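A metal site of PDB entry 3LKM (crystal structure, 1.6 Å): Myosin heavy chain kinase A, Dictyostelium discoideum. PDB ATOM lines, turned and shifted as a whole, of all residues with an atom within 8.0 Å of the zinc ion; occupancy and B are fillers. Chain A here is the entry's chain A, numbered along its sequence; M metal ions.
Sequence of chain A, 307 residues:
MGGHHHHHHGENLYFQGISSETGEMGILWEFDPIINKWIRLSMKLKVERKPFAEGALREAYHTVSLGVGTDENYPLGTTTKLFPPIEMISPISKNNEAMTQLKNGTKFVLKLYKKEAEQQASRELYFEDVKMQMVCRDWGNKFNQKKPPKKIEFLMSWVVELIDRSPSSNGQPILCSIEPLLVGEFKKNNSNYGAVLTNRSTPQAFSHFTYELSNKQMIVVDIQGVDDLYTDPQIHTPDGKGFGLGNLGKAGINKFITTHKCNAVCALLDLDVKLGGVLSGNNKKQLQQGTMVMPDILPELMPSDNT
Within 4 Å of the zinc ion: His 208, His 260, Cys 262 and Cys 266. The nearest printed residue that does not touch the zinc ion is Asn 263 (4.6 Å).
NE2 of His 208 sits close to O of Asp 272, at 3.5 Å. N of Cys 266 lies within hydrogen-bond range of OD1 of Asn 263, at 3.0 Å. The backbone carbonyl oxygen (O) of Cys 266 sits at hydrogen-bond distance from the backbone NH (N) of Leu 271 (3.1 Å).
The zinc ion is bound by a ring nitrogen (NE2) of His 260, a ring nitrogen (ND1) of His 208, the side-chain sulfur (SG) of Cys 266 and the side-chain sulfur (SG) of Cys 262. The zinc ion has four donor atoms within binding distance.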
ATOM      1  N   SER A 201     -12.162  12.254  -2.381  1.00  0.00           N
ATOM      2  CA  SER A 201     -13.009  13.332  -1.867  1.00  0.00           C
ATOM      3  C   SER A 201     -14.313  13.506  -2.648  1.00  0.00           C
ATOM      4  O   SER A 201     -15.377  13.653  -2.073  1.00  0.00           O
ATOM      5  CB  SER A 201     -12.280  14.671  -1.904  1.00  0.00           C
ATOM      6  OG  SER A 201     -11.199  14.696  -1.003  1.00  0.00           O
ATOM      7  N   GLN A 204     -17.680  11.614  -1.908  1.00  0.00           N
ATOM      8  CA  GLN A 204     -18.249  11.871  -0.586  1.00  0.00           C
ATOM      9  C   GLN A 204     -18.765  13.299  -0.505  1.00  0.00           C
ATOM     10  O   GLN A 204     -19.776  13.559   0.143  1.00  0.00           O
ATOM     11  CB  GLN A 204     -17.231  11.616   0.530  1.00  0.00           C
ATOM     12  CG  GLN A 204     -16.531  10.258   0.450  1.00  0.00           C
ATOM     13  CD  GLN A 204     -17.480   9.080   0.318  1.00  0.00           C
ATOM     14  OE1 GLN A 204     -18.577   9.054   0.889  1.00  0.00           O
ATOM     15  NE2 GLN A 204     -17.047   8.070  -0.435  1.00  0.00           N
ATOM     16  N   ALA A 205     -18.051  14.221  -1.148  1.00  0.00           N
ATOM     17  CA  ALA A 205     -18.473  15.625  -1.162  1.00  0.00           C
ATOM     18  C   ALA A 205     -19.754  15.786  -1.958  1.00  0.00           C
ATOM     19  O   ALA A 205     -20.632  16.559  -1.586  1.00  0.00           O
ATOM     20  CB  ALA A 205     -17.376  16.517  -1.705  1.00  0.00           C
ATOM     21  N   PHE A 206     -19.867  15.045  -3.060  1.00  0.00           N
ATOM     22  CA  PHE A 206     -21.106  15.061  -3.829  1.00  0.00           C
ATOM     23  C   PHE A 206     -22.281  14.585  -2.977  1.00  0.00           C
ATOM     24  O   PHE A 206     -23.333  15.243  -2.916  1.00  0.00           O
ATOM     25  CB  PHE A 206     -21.005  14.205  -5.083  1.00  0.00           C
ATOM     26  CG  PHE A 206     -22.312  14.042  -5.794  1.00  0.00           C
ATOM     27  CD1 PHE A 206     -22.886  15.129  -6.446  1.00  0.00           C
ATOM     28  CD2 PHE A 206     -22.987  12.842  -5.768  1.00  0.00           C
ATOM     29  CE1 PHE A 206     -24.109  15.005  -7.077  1.00  0.00           C
ATOM     30  CE2 PHE A 206     -24.206  12.699  -6.410  1.00  0.00           C
ATOM     31  CZ  PHE A 206     -24.773  13.789  -7.074  1.00  0.00           C
ATOM     32  N   SER A 207     -22.126  13.446  -2.308  1.00  0.00           N
ATOM     33  CA  SER A 207     -23.195  12.977  -1.422  1.00  0.00           C
ATOM     34  C   SER A 207     -23.562  14.063  -0.401  1.00  0.00           C
ATOM     35  O   SER A 207     -24.732  14.393  -0.232  1.00  0.00           O
ATOM     36  CB  SER A 207     -22.802  11.669  -0.733  1.00  0.00           C
ATOM     37  OG  SER A 207     -22.684  10.623  -1.672  1.00  0.00           O
ATOM     38  N   HIS A 208     -22.571  14.621   0.289  1.00  0.00           N
ATOM     39  CA  HIS A 208     -22.853  15.669   1.239  1.00  0.00           C
ATOM     40  C   HIS A 208     -23.580  16.859   0.580  1.00  0.00           C
ATOM     41  O   HIS A 208     -24.547  17.386   1.121  1.00  0.00           O
ATOM     42  CB  HIS A 208     -21.568  16.103   1.932  1.00  0.00           C
ATOM     43  CG  HIS A 208     -21.782  17.028   3.077  1.00  0.00           C
ATOM     44  ND1 HIS A 208     -20.753  17.589   3.788  1.00  0.00           N
ATOM     45  CD2 HIS A 208     -22.926  17.521   3.614  1.00  0.00           C
ATOM     46  CE1 HIS A 208     -21.245  18.375   4.732  1.00  0.00           C
ATOM     47  NE2 HIS A 208     -22.566  18.348   4.648  1.00  0.00           N
ATOM     48  N   PHE A 209     -23.100  17.267  -0.597  1.00  0.00           N
ATOM     49  CA  PHE A 209     -23.713  18.355  -1.353  1.00  0.00           C
ATOM     50  C   PHE A 209     -25.201  18.109  -1.548  1.00  0.00           C
ATOM     51  O   PHE A 209     -26.029  18.994  -1.319  1.00  0.00           O
ATOM     52  CB  PHE A 209     -23.010  18.493  -2.707  1.00  0.00           C
ATOM     53  CG  PHE A 209     -23.621  19.524  -3.616  1.00  0.00           C
ATOM     54  CD1 PHE A 209     -23.262  20.855  -3.516  1.00  0.00           C
ATOM     55  CD2 PHE A 209     -24.521  19.144  -4.606  1.00  0.00           C
ATOM     56  CE1 PHE A 209     -23.817  21.809  -4.372  1.00  0.00           C
ATOM     57  CE2 PHE A 209     -25.085  20.094  -5.460  1.00  0.00           C
ATOM     58  CZ  PHE A 209     -24.712  21.429  -5.344  1.00  0.00           C
ATOM     59  N   GLU A 212     -27.168  18.641   1.771  1.00  0.00           N
ATOM     60  CA  GLU A 212     -27.326  20.028   2.206  1.00  0.00           C
ATOM     61  C   GLU A 212     -28.234  20.808   1.273  1.00  0.00           C
ATOM     62  O   GLU A 212     -29.151  21.521   1.699  1.00  0.00           O
ATOM     63  CB  GLU A 212     -25.973  20.729   2.321  1.00  0.00           C
ATOM     64  CG  GLU A 212     -26.084  22.138   2.878  1.00  0.00           C
ATOM     65  CD  GLU A 212     -24.769  22.666   3.414  1.00  0.00           C
ATOM     66  OE1 GLU A 212     -24.486  23.864   3.209  1.00  0.00           O
ATOM     67  OE2 GLU A 212     -24.022  21.881   4.037  1.00  0.00           O
ATOM     68  N   PHE A 256     -25.177   7.543   6.582  1.00  0.00           N
ATOM     69  CA  PHE A 256     -24.223   8.337   5.823  1.00  0.00           C
ATOM     70  C   PHE A 256     -23.546   9.344   6.735  1.00  0.00           C
ATOM     71  O   PHE A 256     -22.328   9.531   6.673  1.00  0.00           O
ATOM     72  CB  PHE A 256     -24.882   9.094   4.672  1.00  0.00           C
ATOM     73  CG  PHE A 256     -23.932  10.023   3.969  1.00  0.00           C
ATOM     74  CD1 PHE A 256     -23.048   9.536   3.023  1.00  0.00           C
ATOM     75  CD2 PHE A 256     -23.870  11.370   4.299  1.00  0.00           C
ATOM     76  CE1 PHE A 256     -22.136  10.384   2.385  1.00  0.00           C
ATOM     77  CE2 PHE A 256     -22.968  12.213   3.664  1.00  0.00           C
ATOM     78  CZ  PHE A 256     -22.103  11.709   2.703  1.00  0.00           C
ATOM     79  N   HIS A 260     -19.469  10.037   7.621  1.00  0.00           N
ATOM     80  CA  HIS A 260     -18.972  11.081   6.728  1.00  0.00           C
ATOM     81  C   HIS A 260     -17.950  11.995   7.392  1.00  0.00           C
ATOM     82  O   HIS A 260     -18.210  12.575   8.442  1.00  0.00           O
ATOM     83  CB  HIS A 260     -20.106  11.952   6.148  1.00  0.00           C
ATOM     84  CG  HIS A 260     -19.605  13.011   5.212  1.00  0.00           C
ATOM     85  ND1 HIS A 260     -18.983  12.704   4.014  1.00  0.00           N
ATOM     86  CD2 HIS A 260     -19.600  14.358   5.298  1.00  0.00           C
ATOM     87  CE1 HIS A 260     -18.638  13.827   3.404  1.00  0.00           C
ATOM     88  NE2 HIS A 260     -19.005  14.841   4.160  1.00  0.00           N
ATOM     89  N   LYS A 261     -16.782  12.092   6.778  1.00  0.00           N
ATOM     90  CA  LYS A 261     -15.762  13.060   7.192  1.00  0.00           C
ATOM     91  C   LYS A 261     -15.623  14.107   6.091  1.00  0.00           C
ATOM     92  O   LYS A 261     -15.317  13.773   4.954  1.00  0.00           O
ATOM     93  CB  LYS A 261     -14.413  12.376   7.366  1.00  0.00           C
ATOM     94  CG  LYS A 261     -14.353  11.392   8.517  1.00  0.00           C
ATOM     95  CD  LYS A 261     -13.014  10.680   8.499  1.00  0.00           C
ATOM     96  CE  LYS A 261     -12.868   9.717   9.667  1.00  0.00           C
ATOM     97  NZ  LYS A 261     -11.569   8.994   9.567  1.00  0.00           N
ATOM     98  N   CYS A 262     -15.842  15.379   6.424  1.00  0.00           N
ATOM     99  CA  CYS A 262     -15.683  16.398   5.392  1.00  0.00           C
ATOM    100  C   CYS A 262     -14.251  16.484   4.876  1.00  0.00           C
ATOM    101  O   CYS A 262     -13.295  16.298   5.623  1.00  0.00           O
ATOM    102  CB  CYS A 262     -16.196  17.755   5.868  1.00  0.00           C
ATOM    103  SG  CYS A 262     -18.017  17.876   5.874  1.00  0.00           S
ATOM    104  N   ASN A 263     -14.133  16.772   3.581  1.00  0.00           N
ATOM    105  CA  ASN A 263     -12.850  16.809   2.899  1.00  0.00           C
ATOM    106  C   ASN A 263     -12.635  18.144   2.199  1.00  0.00           C
ATOM    107  O   ASN A 263     -13.409  19.084   2.380  1.00  0.00           O
ATOM    108  CB  ASN A 263     -12.752  15.640   1.910  1.00  0.00           C
ATOM    109  CG  ASN A 263     -13.887  15.652   0.908  1.00  0.00           C
ATOM    110  OD1 ASN A 263     -14.112  16.668   0.253  1.00  0.00           O
ATOM    111  ND2 ASN A 263     -14.614  14.546   0.798  1.00  0.00           N
ATOM    112  N   ALA A 264     -11.561  18.225   1.423  1.00  0.00           N
ATOM    113  CA  ALA A 264     -11.182  19.461   0.737  1.00  0.00           C
ATOM    114  C   ALA A 264     -12.282  19.975  -0.185  1.00  0.00           C
ATOM    115  O   ALA A 264     -12.472  21.184  -0.321  1.00  0.00           O
ATOM    116  CB  ALA A 264      -9.887  19.261  -0.039  1.00  0.00           C
ATOM    117  N   VAL A 265     -13.005  19.056  -0.822  1.00  0.00           N
ATOM    118  CA  VAL A 265     -14.087  19.448  -1.732  1.00  0.00           C
ATOM    119  C   VAL A 265     -15.309  19.953  -0.939  1.00  0.00           C
ATOM    120  O   VAL A 265     -15.934  20.943  -1.314  1.00  0.00           O
ATOM    121  CB  VAL A 265     -14.466  18.312  -2.715  1.00  0.00           C
ATOM    122  CG1 VAL A 265     -15.573  18.761  -3.674  1.00  0.00           C
ATOM    123  CG2 VAL A 265     -13.236  17.874  -3.504  1.00  0.00           C
ATOM    124  N   CYS A 266     -15.641  19.283   0.162  1.00  0.00           N
ATOM    125  CA  CYS A 266     -16.695  19.794   1.047  1.00  0.00           C
ATOM    126  C   CYS A 266     -16.385  21.231   1.443  1.00  0.00           C
ATOM    127  O   CYS A 266     -17.261  22.088   1.418  1.00  0.00           O
ATOM    128  CB  CYS A 266     -16.791  18.948   2.313  1.00  0.00           C
ATOM    129  SG  CYS A 266     -17.384  17.269   2.032  1.00  0.00           S
ATOM    130  N   ALA A 267     -15.123  21.480   1.789  1.00  0.00           N
ATOM    131  CA  ALA A 267     -14.704  22.807   2.225  1.00  0.00           C
ATOM    132  C   ALA A 267     -14.831  23.840   1.100  1.00  0.00           C
ATOM    133  O   ALA A 267     -15.294  24.959   1.338  1.00  0.00           O
ATOM    134  CB  ALA A 267     -13.273  22.768   2.770  1.00  0.00           C
ATOM    135  N   LEU A 271     -19.766  23.495   2.505  1.00  0.00           N
ATOM    136  CA  LEU A 271     -20.772  22.645   3.115  1.00  0.00           C
ATOM    137  C   LEU A 271     -20.645  22.708   4.630  1.00  0.00           C
ATOM    138  O   LEU A 271     -19.545  22.908   5.165  1.00  0.00           O
ATOM    139  CB  LEU A 271     -20.625  21.205   2.602  1.00  0.00           C
ATOM    140  CG  LEU A 271     -20.813  21.044   1.087  1.00  0.00           C
ATOM    141  CD1 LEU A 271     -20.725  19.588   0.662  1.00  0.00           C
ATOM    142  CD2 LEU A 271     -22.143  21.641   0.654  1.00  0.00           C
ATOM    143  N   ASP A 272     -21.767  22.571   5.316  1.00  0.00           N
ATOM    144  CA  ASP A 272     -21.824  22.619   6.786  1.00  0.00           C
ATOM    145  C   ASP A 272     -20.993  21.503   7.404  1.00  0.00           C
ATOM    146  O   ASP A 272     -21.231  20.322   7.152  1.00  0.00           O
ATOM    147  CB  ASP A 272     -23.286  22.535   7.237  1.00  0.00           C
ATOM    148  CG  ASP A 272     -23.442  22.447   8.759  1.00  0.00           C
ATOM    149  OD1 ASP A 272     -22.575  22.966   9.503  1.00  0.00           O
ATOM    150  OD2 ASP A 272     -24.455  21.870   9.212  1.00  0.00           O
ATOM    151  N   VAL A 273     -20.027  21.884   8.233  1.00  0.00           N
ATOM    152  CA  VAL A 273     -19.135  20.928   8.900  1.00  0.00           C
ATOM    153  C   VAL A 273     -19.837  20.118   9.989  1.00  0.00           C
ATOM    154  O   VAL A 273     -20.924  20.476  10.456  1.00  0.00           O
ATOM    155  CB  VAL A 273     -17.899  21.626   9.510  1.00  0.00           C
ATOM    156  CG1 VAL A 273     -16.998  22.170   8.405  1.00  0.00           C
ATOM    157  CG2 VAL A 273     -18.328  22.724  10.484  1.00  0.00           C
HETATM  158 ZN    ZN M   1     -18.718  16.933   3.878  1.00  0.00          ZN
